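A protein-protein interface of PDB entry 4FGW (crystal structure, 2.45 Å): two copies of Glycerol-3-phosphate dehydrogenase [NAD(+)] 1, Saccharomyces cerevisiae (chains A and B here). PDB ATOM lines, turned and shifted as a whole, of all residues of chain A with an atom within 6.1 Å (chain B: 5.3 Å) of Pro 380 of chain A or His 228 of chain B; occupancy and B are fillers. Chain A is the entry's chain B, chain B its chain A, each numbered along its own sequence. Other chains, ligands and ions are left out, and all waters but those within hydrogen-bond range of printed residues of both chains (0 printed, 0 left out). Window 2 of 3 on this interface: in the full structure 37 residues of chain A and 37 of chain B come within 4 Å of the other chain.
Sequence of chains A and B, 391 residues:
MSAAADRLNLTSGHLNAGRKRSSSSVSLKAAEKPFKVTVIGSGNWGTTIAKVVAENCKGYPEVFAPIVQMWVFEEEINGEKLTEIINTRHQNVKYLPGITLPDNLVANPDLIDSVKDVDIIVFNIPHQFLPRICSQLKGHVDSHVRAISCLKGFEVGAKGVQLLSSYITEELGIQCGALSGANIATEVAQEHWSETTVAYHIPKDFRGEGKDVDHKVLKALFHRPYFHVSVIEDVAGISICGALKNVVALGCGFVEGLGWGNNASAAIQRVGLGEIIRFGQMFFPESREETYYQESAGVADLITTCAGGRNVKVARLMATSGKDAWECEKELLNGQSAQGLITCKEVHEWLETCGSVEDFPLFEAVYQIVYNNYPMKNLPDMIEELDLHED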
ATOM      1  N   VAL A 255       3.165 -24.694  -1.920  1.00  0.00           N
ATOM      2  CA  VAL A 255       1.862 -24.914  -1.311  1.00  0.00           C
ATOM      3  C   VAL A 255       1.752 -26.256  -0.539  1.00  0.00           C
ATOM      4  O   VAL A 255       1.168 -26.287   0.542  1.00  0.00           O
ATOM      5  CB  VAL A 255       0.791 -24.641  -2.404  1.00  0.00           C
ATOM      6  CG1 VAL A 255      -0.140 -25.812  -2.660  1.00  0.00           C
ATOM      7  CG2 VAL A 255       0.047 -23.348  -2.128  1.00  0.00           C
ATOM      8  N   TRP A 260      -0.528 -27.226   2.987  1.00  0.00           N
ATOM      9  CA  TRP A 260      -1.871 -26.855   2.537  1.00  0.00           C
ATOM     10  C   TRP A 260      -2.637 -27.971   1.823  1.00  0.00           C
ATOM     11  O   TRP A 260      -3.848 -27.858   1.635  1.00  0.00           O
ATOM     12  CB  TRP A 260      -1.874 -25.518   1.781  1.00  0.00           C
ATOM     13  CG  TRP A 260      -1.355 -24.331   2.551  1.00  0.00           C
ATOM     14  CD1 TRP A 260      -1.045 -24.273   3.881  1.00  0.00           C
ATOM     15  CD2 TRP A 260      -1.124 -23.013   2.030  1.00  0.00           C
ATOM     16  NE1 TRP A 260      -0.593 -23.017   4.209  1.00  0.00           N
ATOM     17  CE2 TRP A 260      -0.650 -22.217   3.097  1.00  0.00           C
ATOM     18  CE3 TRP A 260      -1.302 -22.419   0.770  1.00  0.00           C
ATOM     19  CZ2 TRP A 260      -0.334 -20.864   2.935  1.00  0.00           C
ATOM     20  CZ3 TRP A 260      -0.951 -21.091   0.604  1.00  0.00           C
ATOM     21  CH2 TRP A 260      -0.489 -20.323   1.681  1.00  0.00           C
ATOM     22  N   MET A 376       5.970 -16.384   0.431  1.00  0.00           N
ATOM     23  CA  MET A 376       5.479 -17.730   0.059  1.00  0.00           C
ATOM     24  C   MET A 376       4.063 -18.010   0.579  1.00  0.00           C
ATOM     25  O   MET A 376       3.255 -18.584  -0.153  1.00  0.00           O
ATOM     26  CB  MET A 376       6.462 -18.841   0.482  1.00  0.00           C
ATOM     27  CG  MET A 376       6.363 -20.104  -0.328  1.00  0.00           C
ATOM     28  SD  MET A 376       7.404 -21.427   0.356  1.00  0.00           S
ATOM     29  CE  MET A 376       8.983 -21.015  -0.338  1.00  0.00           C
ATOM     30  N   LYS A 377       3.762 -17.596   1.829  1.00  0.00           N
ATOM     31  CA  LYS A 377       2.445 -17.737   2.463  1.00  0.00           C
ATOM     32  C   LYS A 377       1.451 -16.767   1.805  1.00  0.00           C
ATOM     33  O   LYS A 377       0.245 -16.960   1.919  1.00  0.00           O
ATOM     34  CB  LYS A 377       2.527 -17.420   3.974  1.00  0.00           C
ATOM     35  CG  LYS A 377       3.484 -18.300   4.782  1.00  0.00           C
ATOM     36  CD  LYS A 377       3.411 -18.019   6.290  1.00  0.00           C
ATOM     37  CE  LYS A 377       4.198 -16.798   6.725  1.00  0.00           C
ATOM     38  NZ  LYS A 377       3.957 -16.460   8.154  1.00  0.00           N
ATOM     39  N   ASN A 378       1.966 -15.715   1.141  1.00  0.00           N
ATOM     40  CA  ASN A 378       1.189 -14.677   0.459  1.00  0.00           C
ATOM     41  C   ASN A 378       0.702 -15.094  -0.933  1.00  0.00           C
ATOM     42  O   ASN A 378      -0.004 -14.317  -1.579  1.00  0.00           O
ATOM     43  CB  ASN A 378       2.005 -13.387   0.362  1.00  0.00           C
ATOM     44  CG  ASN A 378       2.355 -12.719   1.670  1.00  0.00           C
ATOM     45  OD1 ASN A 378       3.210 -11.835   1.709  1.00  0.00           O
ATOM     46  ND2 ASN A 378       1.689 -13.083   2.759  1.00  0.00           N
ATOM     47  N   LEU A 379       1.078 -16.316  -1.388  1.00  0.00           N
ATOM     48  CA  LEU A 379       0.699 -16.893  -2.681  1.00  0.00           C
ATOM     49  C   LEU A 379      -0.806 -16.731  -3.015  1.00  0.00           C
ATOM     50  O   LEU A 379      -1.082 -16.154  -4.069  1.00  0.00           O
ATOM     51  CB  LEU A 379       1.205 -18.347  -2.805  1.00  0.00           C
ATOM     52  CG  LEU A 379       1.354 -18.970  -4.201  1.00  0.00           C
ATOM     53  CD1 LEU A 379       2.237 -18.146  -5.096  1.00  0.00           C
ATOM     54  CD2 LEU A 379       1.966 -20.343  -4.094  1.00  0.00           C
ATOM     55  N   PRO A 380      -1.778 -17.098  -2.118  1.00  0.00           N
ATOM     56  CA  PRO A 380      -3.204 -16.858  -2.429  1.00  0.00           C
ATOM     57  C   PRO A 380      -3.563 -15.398  -2.720  1.00  0.00           C
ATOM     58  O   PRO A 380      -4.338 -15.147  -3.642  1.00  0.00           O
ATOM     59  CB  PRO A 380      -3.926 -17.346  -1.164  1.00  0.00           C
ATOM     60  CG  PRO A 380      -3.010 -18.327  -0.566  1.00  0.00           C
ATOM     61  CD  PRO A 380      -1.645 -17.769  -0.806  1.00  0.00           C
ATOM     62  N   ASP A 381      -3.004 -14.446  -1.940  1.00  0.00           N
ATOM     63  CA  ASP A 381      -3.221 -13.001  -2.094  1.00  0.00           C
ATOM     64  C   ASP A 381      -2.644 -12.473  -3.413  1.00  0.00           C
ATOM     65  O   ASP A 381      -3.213 -11.553  -4.006  1.00  0.00           O
ATOM     66  CB  ASP A 381      -2.605 -12.228  -0.913  1.00  0.00           C
ATOM     67  CG  ASP A 381      -3.184 -12.520   0.466  1.00  0.00           C
ATOM     68  OD1 ASP A 381      -4.342 -12.998   0.542  1.00  0.00           O
ATOM     69  OD2 ASP A 381      -2.503 -12.219   1.471  1.00  0.00           O
ATOM     70  N   MET A 382      -1.509 -13.046  -3.858  1.00  0.00           N
ATOM     71  CA  MET A 382      -0.815 -12.658  -5.091  1.00  0.00           C
ATOM     72  C   MET A 382      -1.587 -13.071  -6.344  1.00  0.00           C
ATOM     73  O   MET A 382      -1.602 -12.331  -7.329  1.00  0.00           O
ATOM     74  CB  MET A 382       0.610 -13.246  -5.128  1.00  0.00           C
ATOM     75  CG  MET A 382       1.525 -12.684  -4.062  1.00  0.00           C
ATOM     76  SD  MET A 382       3.258 -13.158  -4.282  1.00  0.00           S
ATOM     77  CE  MET A 382       3.289 -14.684  -3.502  1.00  0.00           C
ATOM     78  N   ILE A 383      -2.237 -14.246  -6.301  1.00  0.00           N
ATOM     79  CA  ILE A 383      -2.999 -14.790  -7.431  1.00  0.00           C
ATOM     80  C   ILE A 383      -4.507 -14.456  -7.397  1.00  0.00           C
ATOM     81  O   ILE A 383      -5.192 -14.653  -8.407  1.00  0.00           O
ATOM     82  CB  ILE A 383      -2.705 -16.298  -7.655  1.00  0.00           C
ATOM     83  CG1 ILE A 383      -3.295 -17.183  -6.507  1.00  0.00           C
ATOM     84  CG2 ILE A 383      -1.198 -16.520  -7.860  1.00  0.00           C
ATOM     85  CD1 ILE A 383      -3.224 -18.709  -6.737  1.00  0.00           C
ATOM     86  N   GLU A 384      -5.000 -13.948  -6.241  1.00  0.00           N
ATOM     87  CA  GLU A 384      -6.394 -13.569  -5.991  1.00  0.00           C
ATOM     88  C   GLU A 384      -6.952 -12.662  -7.102  1.00  0.00           C
ATOM     89  O   GLU A 384      -6.332 -11.662  -7.467  1.00  0.00           O
ATOM     90  CB  GLU A 384      -6.525 -12.905  -4.612  1.00  0.00           C
ATOM     91  CG  GLU A 384      -7.948 -12.711  -4.112  1.00  0.00           C
ATOM     92  CD  GLU A 384      -8.071 -12.143  -2.708  1.00  0.00           C
ATOM     93  OE1 GLU A 384      -7.186 -11.360  -2.293  1.00  0.00           O
ATOM     94  OE2 GLU A 384      -9.068 -12.465  -2.026  1.00  0.00           O
ATOM     95  N   GLU A 385      -8.108 -13.064  -7.652  1.00  0.00           N
ATOM     96  CA  GLU A 385      -8.842 -12.393  -8.729  1.00  0.00           C
ATOM     97  C   GLU A 385     -10.016 -11.590  -8.148  1.00  0.00           C
ATOM     98  O   GLU A 385     -10.651 -12.019  -7.184  1.00  0.00           O
ATOM     99  CB  GLU A 385      -9.313 -13.454  -9.745  1.00  0.00           C
ATOM    100  CG  GLU A 385     -10.386 -13.037 -10.735  1.00  0.00           C
ATOM    101  CD  GLU A 385     -11.040 -14.227 -11.410  1.00  0.00           C
ATOM    102  OE1 GLU A 385     -12.062 -14.727 -10.884  1.00  0.00           O
ATOM    103  OE2 GLU A 385     -10.499 -14.690 -12.440  1.00  0.00           O
ATOM    104  N   TRP B 193      -6.214 -22.557   2.744  1.00  0.00           N
ATOM    105  CA  TRP B 193      -6.538 -22.062   1.412  1.00  0.00           C
ATOM    106  C   TRP B 193      -6.937 -23.114   0.359  1.00  0.00           C
ATOM    107  O   TRP B 193      -6.212 -24.075   0.099  1.00  0.00           O
ATOM    108  CB  TRP B 193      -5.476 -21.083   0.886  1.00  0.00           C
ATOM    109  CG  TRP B 193      -5.828 -20.523  -0.457  1.00  0.00           C
ATOM    110  CD1 TRP B 193      -6.761 -19.566  -0.727  1.00  0.00           C
ATOM    111  CD2 TRP B 193      -5.334 -20.973  -1.726  1.00  0.00           C
ATOM    112  NE1 TRP B 193      -6.838 -19.351  -2.083  1.00  0.00           N
ATOM    113  CE2 TRP B 193      -5.965 -20.197  -2.721  1.00  0.00           C
ATOM    114  CE3 TRP B 193      -4.386 -21.937  -2.119  1.00  0.00           C
ATOM    115  CZ2 TRP B 193      -5.674 -20.343  -4.084  1.00  0.00           C
ATOM    116  CZ3 TRP B 193      -4.093 -22.080  -3.469  1.00  0.00           C
ATOM    117  CH2 TRP B 193      -4.721 -21.277  -4.434  1.00  0.00           C
ATOM    118  N   SER B 194      -8.093 -22.886  -0.250  1.00  0.00           N
ATOM    119  CA  SER B 194      -8.666 -23.675  -1.333  1.00  0.00           C
ATOM    120  C   SER B 194      -9.578 -22.759  -2.156  1.00  0.00           C
ATOM    121  O   SER B 194      -9.687 -21.561  -1.863  1.00  0.00           O
ATOM    122  CB  SER B 194      -9.425 -24.899  -0.811  1.00  0.00           C
ATOM    123  OG  SER B 194     -10.539 -24.558   0.000  1.00  0.00           O
ATOM    124  N   GLU B 195     -10.203 -23.316  -3.206  1.00  0.00           N
ATOM    125  CA  GLU B 195     -11.092 -22.570  -4.081  1.00  0.00           C
ATOM    126  C   GLU B 195     -12.424 -23.283  -4.235  1.00  0.00           C
ATOM    127  O   GLU B 195     -12.554 -24.471  -3.909  1.00  0.00           O
ATOM    128  CB  GLU B 195     -10.468 -22.413  -5.479  1.00  0.00           C
ATOM    129  CG  GLU B 195      -9.139 -21.679  -5.544  1.00  0.00           C
ATOM    130  CD  GLU B 195      -8.605 -21.525  -6.955  1.00  0.00           C
ATOM    131  OE1 GLU B 195      -8.201 -20.399  -7.317  1.00  0.00           O
ATOM    132  OE2 GLU B 195      -8.621 -22.521  -7.710  1.00  0.00           O
ATOM    133  N   THR B 196     -13.404 -22.550  -4.791  1.00  0.00           N
ATOM    134  CA  THR B 196     -14.704 -23.075  -5.180  1.00  0.00           C
ATOM    135  C   THR B 196     -15.266 -22.294  -6.353  1.00  0.00           C
ATOM    136  O   THR B 196     -14.936 -21.117  -6.547  1.00  0.00           O
ATOM    137  CB  THR B 196     -15.701 -23.213  -4.000  1.00  0.00           C
ATOM    138  OG1 THR B 196     -16.599 -24.274  -4.306  1.00  0.00           O
ATOM    139  CG2 THR B 196     -16.512 -21.935  -3.733  1.00  0.00           C
ATOM    140  N   HIS B 223     -16.923 -15.497  -1.228  1.00  0.00           N
ATOM    141  CA  HIS B 223     -15.482 -15.219  -1.286  1.00  0.00           C
ATOM    142  C   HIS B 223     -14.867 -14.839   0.056  1.00  0.00           C
ATOM    143  O   HIS B 223     -15.390 -13.979   0.772  1.00  0.00           O
ATOM    144  CB  HIS B 223     -15.128 -14.191  -2.372  1.00  0.00           C
ATOM    145  CG  HIS B 223     -13.655 -14.091  -2.640  1.00  0.00           C
ATOM    146  ND1 HIS B 223     -13.045 -14.866  -3.604  1.00  0.00           N
ATOM    147  CD2 HIS B 223     -12.715 -13.334  -2.028  1.00  0.00           C
ATOM    148  CE1 HIS B 223     -11.760 -14.549  -3.558  1.00  0.00           C
ATOM    149  NE2 HIS B 223     -11.514 -13.639  -2.621  1.00  0.00           N
ATOM    150  N   ARG B 224     -13.747 -15.500   0.385  1.00  0.00           N
ATOM    151  CA  ARG B 224     -12.957 -15.267   1.599  1.00  0.00           C
ATOM    152  C   ARG B 224     -11.477 -15.263   1.182  1.00  0.00           C
ATOM    153  O   ARG B 224     -11.164 -15.868   0.157  1.00  0.00           O
ATOM    154  CB  ARG B 224     -13.201 -16.382   2.653  1.00  0.00           C
ATOM    155  CG  ARG B 224     -14.641 -16.558   3.151  1.00  0.00           C
ATOM    156  CD  ARG B 224     -15.232 -15.342   3.865  1.00  0.00           C
ATOM    157  NE  ARG B 224     -14.536 -15.006   5.109  1.00  0.00           N
ATOM    158  CZ  ARG B 224     -13.988 -13.826   5.372  1.00  0.00           C
ATOM    159  NH1 ARG B 224     -14.049 -12.843   4.481  1.00  0.00           N
ATOM    160  NH2 ARG B 224     -13.377 -13.615   6.528  1.00  0.00           N
ATOM    161  N   PRO B 225     -10.542 -14.646   1.947  1.00  0.00           N
ATOM    162  CA  PRO B 225      -9.118 -14.702   1.546  1.00  0.00           C
ATOM    163  C   PRO B 225      -8.559 -16.135   1.489  1.00  0.00           C
ATOM    164  O   PRO B 225      -7.695 -16.430   0.659  1.00  0.00           O
ATOM    165  CB  PRO B 225      -8.412 -13.847   2.608  1.00  0.00           C
ATOM    166  CG  PRO B 225      -9.500 -12.972   3.190  1.00  0.00           C
ATOM    167  CD  PRO B 225     -10.714 -13.854   3.184  1.00  0.00           C
ATOM    168  N   TYR B 226      -9.090 -17.030   2.347  1.00  0.00           N
ATOM    169  CA  TYR B 226      -8.734 -18.449   2.441  1.00  0.00           C
ATOM    170  C   TYR B 226      -9.648 -19.344   1.569  1.00  0.00           C
ATOM    171  O   TYR B 226      -9.482 -20.563   1.553  1.00  0.00           O
ATOM    172  CB  TYR B 226      -8.786 -18.907   3.918  1.00  0.00           C
ATOM    173  CG  TYR B 226     -10.167 -18.838   4.544  1.00  0.00           C
ATOM    174  CD1 TYR B 226     -11.070 -19.892   4.411  1.00  0.00           C
ATOM    175  CD2 TYR B 226     -10.561 -17.732   5.294  1.00  0.00           C
ATOM    176  CE1 TYR B 226     -12.339 -19.835   4.987  1.00  0.00           C
ATOM    177  CE2 TYR B 226     -11.825 -17.668   5.881  1.00  0.00           C
ATOM    178  CZ  TYR B 226     -12.711 -18.723   5.726  1.00  0.00           C
ATOM    179  OH  TYR B 226     -13.961 -18.668   6.299  1.00  0.00           O
ATOM    180  N   PHE B 227     -10.642 -18.756   0.901  1.00  0.00           N
ATOM    181  CA  PHE B 227     -11.608 -19.509   0.093  1.00  0.00           C
ATOM    182  C   PHE B 227     -11.952 -18.708  -1.153  1.00  0.00           C
ATOM    183  O   PHE B 227     -12.916 -17.926  -1.145  1.00  0.00           O
ATOM    184  CB  PHE B 227     -12.867 -19.795   0.948  1.00  0.00           C
ATOM    185  CG  PHE B 227     -13.868 -20.792   0.418  1.00  0.00           C
ATOM    186  CD1 PHE B 227     -13.479 -22.090   0.091  1.00  0.00           C
ATOM    187  CD2 PHE B 227     -15.219 -20.471   0.350  1.00  0.00           C
ATOM    188  CE1 PHE B 227     -14.418 -23.032  -0.336  1.00  0.00           C
ATOM    189  CE2 PHE B 227     -16.156 -21.417  -0.069  1.00  0.00           C
ATOM    190  CZ  PHE B 227     -15.750 -22.695  -0.392  1.00  0.00           C
ATOM    191  N   HIS B 228     -11.132 -18.872  -2.214  1.00  0.00           N
ATOM    192  CA  HIS B 228     -11.306 -18.146  -3.472  1.00  0.00           C
ATOM    193  C   HIS B 228     -12.546 -18.611  -4.228  1.00  0.00           C
ATOM    194  O   HIS B 228     -12.745 -19.810  -4.419  1.00  0.00           O
ATOM    195  CB  HIS B 228     -10.044 -18.222  -4.345  1.00  0.00           C
ATOM    196  CG  HIS B 228      -8.906 -17.359  -3.883  1.00  0.00           C
ATOM    197  ND1 HIS B 228      -8.901 -16.763  -2.636  1.00  0.00           N
ATOM    198  CD2 HIS B 228      -7.764 -17.034  -4.523  1.00  0.00           C
ATOM    199  CE1 HIS B 228      -7.768 -16.085  -2.565  1.00  0.00           C
ATOM    200  NE2 HIS B 228      -7.049 -16.225  -3.674  1.00  0.00           N
ATOM    201  N   VAL B 229     -13.391 -17.648  -4.626  1.00  0.00           N
ATOM    202  CA  VAL B 229     -14.638 -17.922  -5.322  1.00  0.00           C
ATOM    203  C   VAL B 229     -14.638 -17.364  -6.736  1.00  0.00           C
ATOM    204  O   VAL B 229     -14.294 -16.200  -6.949  1.00  0.00           O
ATOM    205  CB  VAL B 229     -15.875 -17.455  -4.477  1.00  0.00           C
ATOM    206  CG1 VAL B 229     -17.171 -17.458  -5.282  1.00  0.00           C
ATOM    207  CG2 VAL B 229     -16.032 -18.316  -3.225  1.00  0.00           C
ATOM    208  N   SER B 230     -15.031 -18.208  -7.699  1.00  0.00           N
ATOM    209  CA  SER B 230     -15.222 -17.823  -9.094  1.00  0.00           C
ATOM    210  C   SER B 230     -16.710 -18.040  -9.384  1.00  0.00           C
ATOM    211  O   SER B 230     -17.218 -19.141  -9.173  1.00  0.00           O
ATOM    212  CB  SER B 230     -14.359 -18.674 -10.016  1.00  0.00           C
ATOM    213  OG  SER B 230     -14.731 -18.470 -11.369  1.00  0.00           O
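Hydrophobic or aromatic side chains of chain A within 4 Å of the printed part of chain B: Pro 380 and Ile 383. Along chain A the printed residues that touch a printed residue of chain B span positions 380 to 384. Hydrophobic or aromatic side chains of chain B within 4 Å of the printed part of chain A: Trp 193, His 223 and His 228.
Among the printed residues, pairs that only touch across the chains: Pro 380 of chain A with Trp 193 of chain B (3.6 Å), Ile 383 of chain A with Trp 193 of chain B (3.8 Å) and Glu 384 of chain A with His 228 of chain B (3.5 Å).
OE2 of Glu 384 of chain A sits at hydrogen-bond distance from NE2 of His 223 of chain B (2.8 Å). O of Pro 380 of chain A lies within hydrogen-bond range of NE2 of His 228 of chain B, 2.9 Å away.
Of chain B, only Trp 193 (3.6 Å) and His 228 (2.9 Å) come within 4 Å of Pro 380 of chain A. His 228 of chain B touches two residues of chain A. Of the printed residues of chain B, Glu 384 of chain A touches His 223 (2.8 Å) and His 228 (3.5 Å). Of the printed residues of chain A, His 223 of chain B touches Glu 384 (2.8 Å). Of the printed residues of chain B, Ile 383 of chain A touches Trp 193. Met 382 of chain A touches none of the printed residues of chain B. Ser 230 of chain B touches none of the printed residues of chain A.
The indole nitrogen of Trp 193 of chain B is in hydrogen-bond range of a ring nitrogen (ND1) of His 228 of chain B (3.4 Å). The backbone NH (N) of His 228 of chain B lies within hydrogen-bond range of the backbone carbonyl oxygen (O) of Ser 194 of chain B, at 3.1 Å. O of His 228 of chain B is in hydrogen-bond range of N of Thr 196 of chain B, 2.8 Å away. A ring nitrogen (ND1) of His 223 of chain B sits at hydrogen-bond distance from the backbone NH of Val 229 of chain B, at 3.0 Å.
No position is printed for both chains. Of the 5 pairs that touch across the chains among the printed residues, none has its exchanged pair printed and touching as well.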
